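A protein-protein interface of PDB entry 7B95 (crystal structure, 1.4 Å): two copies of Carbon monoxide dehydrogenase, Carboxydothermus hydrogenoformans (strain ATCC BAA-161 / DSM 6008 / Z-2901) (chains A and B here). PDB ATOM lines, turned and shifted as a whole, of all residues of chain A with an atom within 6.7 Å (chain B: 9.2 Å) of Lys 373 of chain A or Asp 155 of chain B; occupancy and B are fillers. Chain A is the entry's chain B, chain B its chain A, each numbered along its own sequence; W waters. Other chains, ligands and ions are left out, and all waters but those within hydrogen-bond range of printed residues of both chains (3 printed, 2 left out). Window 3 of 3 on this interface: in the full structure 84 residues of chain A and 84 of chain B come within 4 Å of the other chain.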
ATOM      1  N   GLU A  97      -0.930 -25.377  34.963  1.00  0.00           N
ATOM      2  CA  GLU A  97      -1.732 -24.310  34.364  1.00  0.00           C
ATOM      3  C   GLU A  97      -1.101 -22.944  34.584  1.00  0.00           C
ATOM      4  O   GLU A  97      -1.143 -22.099  33.699  1.00  0.00           O
ATOM      5  CB  GLU A  97      -3.161 -24.338  34.879  1.00  0.00           C
ATOM      6  CG  GLU A  97      -3.884 -25.587  34.432  1.00  0.00           C
ATOM      7  CD  GLU A  97      -5.371 -25.409  34.200  1.00  0.00           C
ATOM      8  OE1 GLU A  97      -5.989 -24.531  34.843  1.00  0.00           O
ATOM      9  OE2 GLU A  97      -5.931 -26.221  33.416  1.00  0.00           O
ATOM     10  N   LYS A 100       1.792 -22.754  31.983  1.00  0.00           N
ATOM     11  CA  LYS A 100       1.273 -22.519  30.649  1.00  0.00           C
ATOM     12  C   LYS A 100       0.697 -21.115  30.540  1.00  0.00           C
ATOM     13  O   LYS A 100       0.783 -20.495  29.481  1.00  0.00           O
ATOM     14  CB  LYS A 100       0.247 -23.581  30.269  1.00  0.00           C
ATOM     15  CG  LYS A 100       0.879 -24.967  30.121  1.00  0.00           C
ATOM     16  CD  LYS A 100       0.536 -25.750  28.841  1.00  0.00           C
ATOM     17  CE  LYS A 100      -0.907 -25.578  28.381  1.00  0.00           C
ATOM     18  NZ  LYS A 100      -1.538 -26.862  27.905  1.00  0.00           N
ATOM     19  N   THR A 101       0.090 -20.604  31.614  1.00  0.00           N
ATOM     20  CA  THR A 101      -0.458 -19.255  31.556  1.00  0.00           C
ATOM     21  C   THR A 101       0.662 -18.228  31.438  1.00  0.00           C
ATOM     22  O   THR A 101       0.557 -17.258  30.672  1.00  0.00           O
ATOM     23  CB  THR A 101      -1.322 -18.999  32.795  1.00  0.00           C
ATOM     24  OG1 THR A 101      -2.433 -19.885  32.760  1.00  0.00           O
ATOM     25  CG2 THR A 101      -1.849 -17.607  32.807  1.00  0.00           C
ATOM     26  N   THR A 110      -2.918 -13.615  26.237  1.00  0.00           N
ATOM     27  CA  THR A 110      -3.841 -13.540  27.355  1.00  0.00           C
ATOM     28  C   THR A 110      -4.059 -12.087  27.713  1.00  0.00           C
ATOM     29  O   THR A 110      -3.364 -11.197  27.217  1.00  0.00           O
ATOM     30  CB  THR A 110      -3.280 -14.256  28.584  1.00  0.00           C
ATOM     31  OG1 THR A 110      -2.300 -13.405  29.172  1.00  0.00           O
ATOM     32  CG2 THR A 110      -2.686 -15.616  28.210  1.00  0.00           C
ATOM     33  N   VAL A 357     -15.625 -23.411  35.174  1.00  0.00           N
ATOM     34  CA  VAL A 357     -14.516 -22.895  34.380  1.00  0.00           C
ATOM     35  C   VAL A 357     -13.308 -23.814  34.478  1.00  0.00           C
ATOM     36  O   VAL A 357     -12.180 -23.373  34.296  1.00  0.00           O
ATOM     37  CB  VAL A 357     -14.203 -21.428  34.720  1.00  0.00           C
ATOM     38  CG1 VAL A 357     -15.410 -20.586  34.407  1.00  0.00           C
ATOM     39  CG2 VAL A 357     -13.776 -21.241  36.154  1.00  0.00           C
ATOM     40  N   ARG A 359     -12.162 -28.122  33.526  1.00  0.00           N
ATOM     41  CA  ARG A 359     -12.518 -29.488  33.162  1.00  0.00           C
ATOM     42  C   ARG A 359     -12.614 -30.405  34.381  1.00  0.00           C
ATOM     43  O   ARG A 359     -13.234 -31.473  34.297  1.00  0.00           O
ATOM     44  CB  ARG A 359     -11.618 -30.024  32.074  1.00  0.00           C
ATOM     45  CG  ARG A 359     -10.290 -30.362  32.510  1.00  0.00           C
ATOM     46  CD  ARG A 359      -9.585 -31.081  31.389  1.00  0.00           C
ATOM     47  NE  ARG A 359      -8.202 -31.319  31.722  1.00  0.00           N
ATOM     48  CZ  ARG A 359      -7.254 -30.399  31.591  1.00  0.00           C
ATOM     49  NH1 ARG A 359      -7.562 -29.185  31.129  1.00  0.00           N
ATOM     50  NH2 ARG A 359      -6.004 -30.697  31.917  1.00  0.00           N
ATOM     51  N   LEU A 370     -17.306 -23.703  30.639  1.00  0.00           N
ATOM     52  CA  LEU A 370     -16.310 -22.878  29.942  1.00  0.00           C
ATOM     53  C   LEU A 370     -14.940 -23.231  30.487  1.00  0.00           C
ATOM     54  O   LEU A 370     -14.342 -22.445  31.246  1.00  0.00           O
ATOM     55  CB  LEU A 370     -16.585 -21.431  30.161  1.00  0.00           C
ATOM     56  CG  LEU A 370     -17.988 -20.948  29.846  1.00  0.00           C
ATOM     57  CD1 LEU A 370     -18.094 -19.488  30.202  1.00  0.00           C
ATOM     58  CD2 LEU A 370     -18.328 -21.187  28.411  1.00  0.00           C
ATOM     59  N   ASP A 371     -14.471 -24.412  30.120  1.00  0.00           N
ATOM     60  CA  ASP A 371     -13.191 -24.926  30.608  1.00  0.00           C
ATOM     61  C   ASP A 371     -12.066 -23.940  30.281  1.00  0.00           C
ATOM     62  O   ASP A 371     -11.991 -23.368  29.192  1.00  0.00           O
ATOM     63  CB  ASP A 371     -12.818 -26.239  29.917  1.00  0.00           C
ATOM     64  CG  ASP A 371     -13.748 -27.393  30.200  1.00  0.00           C
ATOM     65  OD1 ASP A 371     -14.533 -27.385  31.171  1.00  0.00           O
ATOM     66  OD2 ASP A 371     -13.645 -28.367  29.408  1.00  0.00           O
ATOM     67  N   TYR A 372     -11.159 -23.782  31.202  1.00  0.00           N
ATOM     68  CA  TYR A 372     -10.101 -22.792  31.060  1.00  0.00           C
ATOM     69  C   TYR A 372      -9.032 -23.189  30.052  1.00  0.00           C
ATOM     70  O   TYR A 372      -8.592 -24.342  29.978  1.00  0.00           O
ATOM     71  CB  TYR A 372      -9.426 -22.600  32.418  1.00  0.00           C
ATOM     72  CG  TYR A 372      -8.225 -21.670  32.382  1.00  0.00           C
ATOM     73  CD1 TYR A 372      -8.392 -20.308  32.329  1.00  0.00           C
ATOM     74  CD2 TYR A 372      -6.918 -22.158  32.451  1.00  0.00           C
ATOM     75  CE1 TYR A 372      -7.322 -19.464  32.300  1.00  0.00           C
ATOM     76  CE2 TYR A 372      -5.831 -21.293  32.435  1.00  0.00           C
ATOM     77  CZ  TYR A 372      -6.051 -19.956  32.375  1.00  0.00           C
ATOM     78  OH  TYR A 372      -5.014 -19.055  32.338  1.00  0.00           O
ATOM     79  N   LYS A 373      -8.610 -22.200  29.280  1.00  0.00           N
ATOM     80  CA  LYS A 373      -7.417 -22.287  28.475  1.00  0.00           C
ATOM     81  C   LYS A 373      -6.893 -20.861  28.485  1.00  0.00           C
ATOM     82  O   LYS A 373      -7.687 -19.929  28.344  1.00  0.00           O
ATOM     83  CB  LYS A 373      -7.755 -22.715  27.036  1.00  0.00           C
ATOM     84  CG  LYS A 373      -6.561 -23.077  26.183  1.00  0.00           C
ATOM     85  CD  LYS A 373      -6.994 -23.903  24.978  1.00  0.00           C
ATOM     86  CE  LYS A 373      -5.928 -23.867  23.885  1.00  0.00           C
ATOM     87  NZ  LYS A 373      -6.284 -24.728  22.705  1.00  0.00           N
ATOM     88  N   PRO A 374      -5.582 -20.652  28.634  1.00  0.00           N
ATOM     89  CA  PRO A 374      -5.064 -19.264  28.702  1.00  0.00           C
ATOM     90  C   PRO A 374      -5.466 -18.367  27.543  1.00  0.00           C
ATOM     91  O   PRO A 374      -5.864 -17.224  27.766  1.00  0.00           O
ATOM     92  CB  PRO A 374      -3.548 -19.471  28.795  1.00  0.00           C
ATOM     93  CG  PRO A 374      -3.388 -20.769  29.404  1.00  0.00           C
ATOM     94  CD  PRO A 374      -4.527 -21.630  28.918  1.00  0.00           C
ATOM     95  N   SER A 375      -5.418 -18.869  26.318  1.00  0.00           N
ATOM     96  CA  SER A 375      -5.771 -18.064  25.154  1.00  0.00           C
ATOM     97  C   SER A 375      -7.280 -17.849  25.029  1.00  0.00           C
ATOM     98  O   SER A 375      -7.708 -17.092  24.149  1.00  0.00           O
ATOM     99  CB  SER A 375      -5.202 -18.709  23.887  1.00  0.00           C
ATOM    100  OG  SER A 375      -5.820 -19.958  23.664  1.00  0.00           O
ATOM    101  N   GLU A 376      -8.096 -18.516  25.852  1.00  0.00           N
ATOM    102  CA  GLU A 376      -9.542 -18.360  25.823  1.00  0.00           C
ATOM    103  C   GLU A 376     -10.077 -17.581  27.021  1.00  0.00           C
ATOM    104  O   GLU A 376     -11.267 -17.297  27.062  1.00  0.00           O
ATOM    105  CB  GLU A 376     -10.240 -19.735  25.756  1.00  0.00           C
ATOM    106  CG  GLU A 376      -9.959 -20.520  24.480  1.00  0.00           C
ATOM    107  CD  GLU A 376     -10.763 -21.822  24.385  1.00  0.00           C
ATOM    108  OE1 GLU A 376     -11.399 -22.238  25.372  1.00  0.00           O
ATOM    109  OE2 GLU A 376     -10.733 -22.469  23.320  1.00  0.00           O
ATOM    110  N   VAL A 377      -9.232 -17.214  27.989  1.00  0.00           N
ATOM    111  CA  VAL A 377      -9.745 -16.662  29.244  1.00  0.00           C
ATOM    112  C   VAL A 377     -10.377 -15.288  29.049  1.00  0.00           C
ATOM    113  O   VAL A 377     -11.310 -14.920  29.780  1.00  0.00           O
ATOM    114  CB  VAL A 377      -8.678 -16.696  30.356  1.00  0.00           C
ATOM    115  CG1 VAL A 377      -7.675 -15.592  30.228  1.00  0.00           C
ATOM    116  CG2 VAL A 377      -9.339 -16.606  31.732  1.00  0.00           C
ATOM    117  N   ARG A 378      -9.889 -14.497  28.090  1.00  0.00           N
ATOM    118  CA  ARG A 378     -10.539 -13.218  27.827  1.00  0.00           C
ATOM    119  C   ARG A 378     -11.992 -13.431  27.415  1.00  0.00           C
ATOM    120  O   ARG A 378     -12.914 -12.789  27.938  1.00  0.00           O
ATOM    121  CB  ARG A 378      -9.768 -12.465  26.738  1.00  0.00           C
ATOM    122  CG  ARG A 378     -10.137 -11.010  26.634  1.00  0.00           C
ATOM    123  CD  ARG A 378      -9.556 -10.366  25.369  1.00  0.00           C
ATOM    124  NE  ARG A 378      -8.115 -10.557  25.201  1.00  0.00           N
ATOM    125  CZ  ARG A 378      -7.197  -9.704  25.640  1.00  0.00           C
ATOM    126  NH1 ARG A 378      -7.560  -8.609  26.319  1.00  0.00           N
ATOM    127  NH2 ARG A 378      -5.909  -9.949  25.422  1.00  0.00           N
ATOM    128  N   ILE A 380     -13.749 -16.160  27.974  1.00  0.00           N
ATOM    129  CA  ILE A 380     -14.465 -16.809  29.069  1.00  0.00           C
ATOM    130  C   ILE A 380     -15.009 -15.756  30.021  1.00  0.00           C
ATOM    131  O   ILE A 380     -16.177 -15.777  30.410  1.00  0.00           O
ATOM    132  CB  ILE A 380     -13.549 -17.813  29.792  1.00  0.00           C
ATOM    133  CG1 ILE A 380     -13.305 -19.037  28.920  1.00  0.00           C
ATOM    134  CG2 ILE A 380     -14.168 -18.232  31.140  1.00  0.00           C
ATOM    135  CD1 ILE A 380     -12.156 -19.927  29.342  1.00  0.00           C
ATOM    136  N   TRP B 148       7.558 -38.904  25.042  1.00  0.00           N
ATOM    137  CA  TRP B 148       6.688 -37.768  24.728  1.00  0.00           C
ATOM    138  C   TRP B 148       5.211 -38.159  24.774  1.00  0.00           C
ATOM    139  O   TRP B 148       4.382 -37.409  25.304  1.00  0.00           O
ATOM    140  CB  TRP B 148       7.062 -37.148  23.363  1.00  0.00           C
ATOM    141  CG  TRP B 148       6.030 -36.162  22.857  1.00  0.00           C
ATOM    142  CD1 TRP B 148       5.887 -34.854  23.242  1.00  0.00           C
ATOM    143  CD2 TRP B 148       4.952 -36.426  21.942  1.00  0.00           C
ATOM    144  NE1 TRP B 148       4.797 -34.293  22.606  1.00  0.00           N
ATOM    145  CE2 TRP B 148       4.210 -35.238  21.806  1.00  0.00           C
ATOM    146  CE3 TRP B 148       4.550 -37.553  21.221  1.00  0.00           C
ATOM    147  CZ2 TRP B 148       3.102 -35.136  20.956  1.00  0.00           C
ATOM    148  CZ3 TRP B 148       3.444 -37.453  20.386  1.00  0.00           C
ATOM    149  CH2 TRP B 148       2.737 -36.253  20.257  1.00  0.00           C
ATOM    150  N   TYR B 151       3.960 -38.056  28.253  1.00  0.00           N
ATOM    151  CA  TYR B 151       3.916 -36.735  28.875  1.00  0.00           C
ATOM    152  C   TYR B 151       2.995 -35.735  28.182  1.00  0.00           C
ATOM    153  O   TYR B 151       2.847 -34.610  28.676  1.00  0.00           O
ATOM    154  CB  TYR B 151       5.302 -36.114  28.860  1.00  0.00           C
ATOM    155  CG  TYR B 151       6.243 -36.521  29.945  1.00  0.00           C
ATOM    156  CD1 TYR B 151       6.119 -36.031  31.216  1.00  0.00           C
ATOM    157  CD2 TYR B 151       7.318 -37.323  29.671  1.00  0.00           C
ATOM    158  CE1 TYR B 151       7.032 -36.364  32.216  1.00  0.00           C
ATOM    159  CE2 TYR B 151       8.221 -37.665  30.648  1.00  0.00           C
ATOM    160  CZ  TYR B 151       8.080 -37.176  31.906  1.00  0.00           C
ATOM    161  OH  TYR B 151       8.996 -37.515  32.845  1.00  0.00           O
ATOM    162  N   ARG B 152       2.394 -36.083  27.047  1.00  0.00           N
ATOM    163  CA  ARG B 152       1.550 -35.158  26.293  1.00  0.00           C
ATOM    164  C   ARG B 152       0.381 -34.654  27.136  1.00  0.00           C
ATOM    165  O   ARG B 152      -0.246 -35.428  27.843  1.00  0.00           O
ATOM    166  CB  ARG B 152       0.936 -35.983  25.138  1.00  0.00           C
ATOM    167  CG  ARG B 152       1.001 -35.400  23.772  1.00  0.00           C
ATOM    168  CD  ARG B 152       0.179 -36.178  22.729  1.00  0.00           C
ATOM    169  NE  ARG B 152      -0.502 -37.395  23.184  1.00  0.00           N
ATOM    170  CZ  ARG B 152      -1.780 -37.455  23.562  1.00  0.00           C
ATOM    171  NH1 ARG B 152      -2.548 -36.370  23.571  1.00  0.00           N
ATOM    172  NH2 ARG B 152      -2.292 -38.612  23.948  1.00  0.00           N
ATOM    173  N   ASP B 153       0.068 -33.354  27.048  1.00  0.00           N
ATOM    174  CA  ASP B 153      -1.053 -32.789  27.811  1.00  0.00           C
ATOM    175  C   ASP B 153      -2.368 -32.864  27.030  1.00  0.00           C
ATOM    176  O   ASP B 153      -2.415 -33.315  25.891  1.00  0.00           O
ATOM    177  CB  ASP B 153      -0.714 -31.392  28.367  1.00  0.00           C
ATOM    178  CG  ASP B 153      -0.699 -30.287  27.321  1.00  0.00           C
ATOM    179  OD1 ASP B 153      -1.292 -30.433  26.237  1.00  0.00           O
ATOM    180  OD2 ASP B 153      -0.091 -29.232  27.627  1.00  0.00           O
ATOM    181  N   TYR B 154      -3.474 -32.468  27.677  1.00  0.00           N
ATOM    182  CA  TYR B 154      -4.790 -32.764  27.121  1.00  0.00           C
ATOM    183  C   TYR B 154      -5.035 -32.029  25.820  1.00  0.00           C
ATOM    184  O   TYR B 154      -5.965 -32.394  25.096  1.00  0.00           O
ATOM    185  CB  TYR B 154      -5.921 -32.389  28.099  1.00  0.00           C
ATOM    186  CG  TYR B 154      -6.296 -30.929  28.050  1.00  0.00           C
ATOM    187  CD1 TYR B 154      -5.526 -29.978  28.707  1.00  0.00           C
ATOM    188  CD2 TYR B 154      -7.402 -30.488  27.331  1.00  0.00           C
ATOM    189  CE1 TYR B 154      -5.847 -28.633  28.660  1.00  0.00           C
ATOM    190  CE2 TYR B 154      -7.730 -29.157  27.282  1.00  0.00           C
ATOM    191  CZ  TYR B 154      -6.945 -28.229  27.937  1.00  0.00           C
ATOM    192  OH  TYR B 154      -7.268 -26.895  27.885  1.00  0.00           O
ATOM    193  N   ASP B 155      -4.204 -31.039  25.506  1.00  0.00           N
ATOM    194  CA  ASP B 155      -4.434 -30.133  24.386  1.00  0.00           C
ATOM    195  C   ASP B 155      -3.434 -30.305  23.248  1.00  0.00           C
ATOM    196  O   ASP B 155      -3.431 -29.479  22.327  1.00  0.00           O
ATOM    197  CB  ASP B 155      -4.401 -28.682  24.888  1.00  0.00           C
ATOM    198  CG  ASP B 155      -5.045 -27.711  23.931  1.00  0.00           C
ATOM    199  OD1 ASP B 155      -6.136 -28.029  23.395  1.00  0.00           O
ATOM    200  OD2 ASP B 155      -4.471 -26.618  23.743  1.00  0.00           O
ATOM    201  N   GLU B 156      -2.612 -31.358  23.267  1.00  0.00           N
ATOM    202  CA  GLU B 156      -1.658 -31.673  22.191  1.00  0.00           C
ATOM    203  C   GLU B 156      -2.026 -33.026  21.578  1.00  0.00           C
ATOM    204  O   GLU B 156      -2.126 -34.009  22.320  1.00  0.00           O
ATOM    205  CB  GLU B 156      -0.244 -31.751  22.808  1.00  0.00           C
ATOM    206  CG  GLU B 156       0.909 -31.853  21.822  1.00  0.00           C
ATOM    207  CD  GLU B 156       2.283 -31.794  22.508  1.00  0.00           C
ATOM    208  OE1 GLU B 156       2.354 -31.875  23.760  1.00  0.00           O
ATOM    209  OE2 GLU B 156       3.296 -31.663  21.775  1.00  0.00           O
ATOM    210  N   PRO B 157      -2.238 -33.147  20.256  1.00  0.00           N
ATOM    211  CA  PRO B 157      -2.753 -34.421  19.711  1.00  0.00           C
ATOM    212  C   PRO B 157      -1.738 -35.560  19.747  1.00  0.00           C
ATOM    213  O   PRO B 157      -0.545 -35.370  19.510  1.00  0.00           O
ATOM    214  CB  PRO B 157      -3.117 -34.081  18.263  1.00  0.00           C
ATOM    215  CG  PRO B 157      -3.130 -32.639  18.181  1.00  0.00           C
ATOM    216  CD  PRO B 157      -2.153 -32.127  19.197  1.00  0.00           C
ATOM    217  N   GLY B 158      -2.241 -36.765  20.005  1.00  0.00           N
ATOM    218  CA  GLY B 158      -1.386 -37.929  20.030  1.00  0.00           C
ATOM    219  C   GLY B 158      -1.211 -38.508  18.644  1.00  0.00           C
ATOM    220  O   GLY B 158      -2.008 -38.215  17.766  1.00  0.00           O
ATOM    221  N   TYR B 179     -10.912 -38.182  23.335  1.00  0.00           N
ATOM    222  CA  TYR B 179      -9.480 -38.328  23.048  1.00  0.00           C
ATOM    223  C   TYR B 179      -8.673 -37.861  24.254  1.00  0.00           C
ATOM    224  O   TYR B 179      -8.813 -36.708  24.670  1.00  0.00           O
ATOM    225  CB  TYR B 179      -9.056 -37.481  21.846  1.00  0.00           C
ATOM    226  CG  TYR B 179      -9.047 -38.222  20.536  1.00  0.00           C
ATOM    227  CD1 TYR B 179      -8.000 -39.020  20.164  1.00  0.00           C
ATOM    228  CD2 TYR B 179     -10.110 -38.153  19.708  1.00  0.00           C
ATOM    229  CE1 TYR B 179      -8.007 -39.699  18.946  1.00  0.00           C
ATOM    230  CE2 TYR B 179     -10.117 -38.804  18.514  1.00  0.00           C
ATOM    231  CZ  TYR B 179      -9.093 -39.578  18.133  1.00  0.00           C
ATOM    232  OH  TYR B 179      -9.227 -40.179  16.895  1.00  0.00           O
ATOM    233  N   PRO B 180      -7.798 -38.685  24.815  1.00  0.00           N
ATOM    234  CA  PRO B 180      -7.170 -38.319  26.094  1.00  0.00           C
ATOM    235  C   PRO B 180      -5.841 -37.608  25.922  1.00  0.00           C
ATOM    236  O   PRO B 180      -5.253 -37.594  24.849  1.00  0.00           O
ATOM    237  CB  PRO B 180      -6.930 -39.671  26.760  1.00  0.00           C
ATOM    238  CG  PRO B 180      -6.672 -40.580  25.587  1.00  0.00           C
ATOM    239  CD  PRO B 180      -7.559 -40.104  24.463  1.00  0.00           C
ATOM    240  N   ALA B 181      -5.395 -37.003  27.018  1.00  0.00           N
ATOM    241  CA  ALA B 181      -4.016 -36.590  27.185  1.00  0.00           C
ATOM    242  C   ALA B 181      -3.127 -37.829  27.205  1.00  0.00           C
ATOM    243  O   ALA B 181      -3.609 -38.964  27.132  1.00  0.00           O
ATOM    244  CB  ALA B 181      -3.875 -35.849  28.515  1.00  0.00           C
ATOM    245  N   GLY B 182      -1.833 -37.632  27.299  1.00  0.00           N
ATOM    246  CA  GLY B 182      -0.946 -38.722  27.616  1.00  0.00           C
ATOM    247  C   GLY B 182      -1.303 -39.228  28.993  1.00  0.00           C
ATOM    248  O   GLY B 182      -1.978 -38.539  29.762  1.00  0.00           O
ATOM    249  N   HIS B 185      -0.588 -37.023  32.389  1.00  0.00           N
ATOM    250  CA  HIS B 185      -1.560 -35.958  32.612  1.00  0.00           C
ATOM    251  C   HIS B 185      -2.952 -36.507  32.851  1.00  0.00           C
ATOM    252  O   HIS B 185      -3.682 -35.991  33.714  1.00  0.00           O
ATOM    253  CB  HIS B 185      -1.582 -34.983  31.442  1.00  0.00           C
ATOM    254  CG  HIS B 185      -0.548 -33.910  31.542  1.00  0.00           C
ATOM    255  ND1 HIS B 185      -0.682 -32.840  32.404  1.00  0.00           N
ATOM    256  CD2 HIS B 185       0.652 -33.745  30.923  1.00  0.00           C
ATOM    257  CE1 HIS B 185       0.385 -32.060  32.294  1.00  0.00           C
ATOM    258  NE2 HIS B 185       1.209 -32.593  31.413  1.00  0.00           N
ATOM    259  N   GLU B 186      -3.352 -37.543  32.110  1.00  0.00           N
ATOM    260  CA  GLU B 186      -4.709 -38.044  32.277  1.00  0.00           C
ATOM    261  C   GLU B 186      -4.923 -38.612  33.684  1.00  0.00           C
ATOM    262  O   GLU B 186      -5.966 -38.388  34.303  1.00  0.00           O
ATOM    263  CB  GLU B 186      -5.042 -39.070  31.210  1.00  0.00           C
ATOM    264  CG  GLU B 186      -6.505 -39.299  31.091  1.00  0.00           C
ATOM    265  CD  GLU B 186      -7.262 -38.110  30.477  1.00  0.00           C
ATOM    266  OE1 GLU B 186      -8.430 -38.012  30.751  1.00  0.00           O
ATOM    267  OE2 GLU B 186      -6.727 -37.311  29.690  1.00  0.00           O
ATOM    268  N   ASP B 189      -5.119 -35.759  36.125  1.00  0.00           N
ATOM    269  CA  ASP B 189      -6.399 -35.081  36.004  1.00  0.00           C
ATOM    270  C   ASP B 189      -7.498 -35.909  36.641  1.00  0.00           C
ATOM    271  O   ASP B 189      -8.395 -35.357  37.288  1.00  0.00           O
ATOM    272  CB  ASP B 189      -6.736 -34.836  34.545  1.00  0.00           C
ATOM    273  CG  ASP B 189      -5.844 -33.788  33.881  1.00  0.00           C
ATOM    274  OD1 ASP B 189      -5.006 -33.171  34.583  1.00  0.00           O
ATOM    275  OD2 ASP B 189      -5.996 -33.618  32.639  1.00  0.00           O
ATOM    276  N   ARG B 211     -11.722 -42.214  29.130  1.00  0.00           N
ATOM    277  CA  ARG B 211     -10.516 -41.505  28.685  1.00  0.00           C
ATOM    278  C   ARG B 211      -9.252 -42.116  29.279  1.00  0.00           C
ATOM    279  O   ARG B 211      -8.227 -42.263  28.586  1.00  0.00           O
ATOM    280  CB  ARG B 211     -10.567 -40.036  29.098  1.00  0.00           C
ATOM    281  CG  ARG B 211     -11.609 -39.221  28.414  1.00  0.00           C
ATOM    282  CD  ARG B 211     -11.711 -37.829  29.087  1.00  0.00           C
ATOM    283  NE  ARG B 211     -10.427 -37.142  29.032  1.00  0.00           N
ATOM    284  CZ  ARG B 211     -10.092 -36.242  28.123  1.00  0.00           C
ATOM    285  NH1 ARG B 211      -8.870 -35.713  28.130  1.00  0.00           N
ATOM    286  NH2 ARG B 211     -10.979 -35.845  27.207  1.00  0.00           N
HETATM  287  O   HOH W   1      -3.510 -25.616  26.245  1.00  0.00           O
HETATM  288  O   HOH W   2      -6.744 -26.174  30.651  1.00  0.00           O
HETATM  289  O   HOH W   3      -9.766 -26.409  27.867  1.00  0.00           O
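Arg 359 of chain A touches Tyr 154 of chain B.
Tyr 154 of chain B touches Tyr 372 of chain A (OH to O, 3.6 Å).
NH2 of Arg 359 of chain A is in salt-bridge range of OD2 of Asp 189 of chain B, at 3.0 Å.
The side-chain carboxylate (OD2) of Asp 155 of chain B is in salt-bridge range of the side-chain amino group (NZ) of Lys 373 of chain A, at 2.8 Å.
OD2 of Asp 153 of chain B lies within salt-bridge range of NZ of Lys 100 of chain A (2.8 Å).
Water W3 lies within hydrogen-bond range of the side-chain hydroxyl of Tyr 154 of chain B (2.5 Å) and the backbone carbonyl oxygen of Tyr 372 of chain A (3.2 Å).
Water W2 lies within hydrogen-bond range of the backbone carbonyl oxygen of Tyr 372 of chain A, the side-chain carboxylate of Glu 97 of chain A, the side-chain hydroxyl of Tyr 154 of chain B and the guanidinium group of Arg 359 of chain A.
Water W1 bridges the side-chain carboxylate (OD2) of Asp 155 of chain B (2.9 Å) and the side-chain amino group (NZ) of Lys 100 of chain A (2.9 Å).
Of the 17 printed residues of chain B, 4 touch a printed residue of chain A.
Hydrophobic or aromatic side chains of chain B that line the printed part of chain A: Tyr 154.
Among the printed residues, 5 pairs touch across the chains.
No position is printed for both chains.
Of the 5 pairs that touch across the chains among the printed residues, none has its exchanged pair printed and touching as well.
Of the printed residues of chain B, Lys 373 of chain A touches Asp 155.
Of the printed residues of chain A, Asp 155 of chain B touches Lys 373 (2.8 Å).
Tyr 372 of chain A touches just one residue of chain B: Tyr 154 (3.6 Å).
No residue of chain B comes within 4 Å of Pro 374 of chain A.
No residue of chain B comes within 4 Å of Glu 376 of chain A.
Printed residues of chain A within 4 Å of Tyr 154 of chain B: Arg 359 and Tyr 372.
Of the printed residues of chain B, Arg 359 of chain A touches Tyr 154 and Asp 189.
The nearest printed residue of chain A that does not touch Asp 155 of chain B is Lys 100 of chain A (4.5 Å).
The nearest printed residue of chain A that does not touch Asp 153 of chain B is Arg 359 of chain A (6.4 Å).
OD1 of Asp 153 of chain B is in hydrogen-bond range of N of Glu 156 of chain B, 3.4 Å away.
The backbone carbonyl oxygen (O) of Val 357 of chain A lies within hydrogen-bond range of the backbone NH (N) of Tyr 372 of chain A (3.3 Å).
The side-chain carboxylate of Asp 371 of chain A is in hydrogen-bond range of the backbone NH of Arg 359 of chain A.
The side-chain hydroxyl (OG1) of Thr 101 of chain A sits at hydrogen-bond distance from the side-chain hydroxyl (OH) of Tyr 372 of chain A, 2.7 Å away.
N of Asp 155 of chain B lies close to OD1 of Asp 153 of chain B (3.1 Å).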
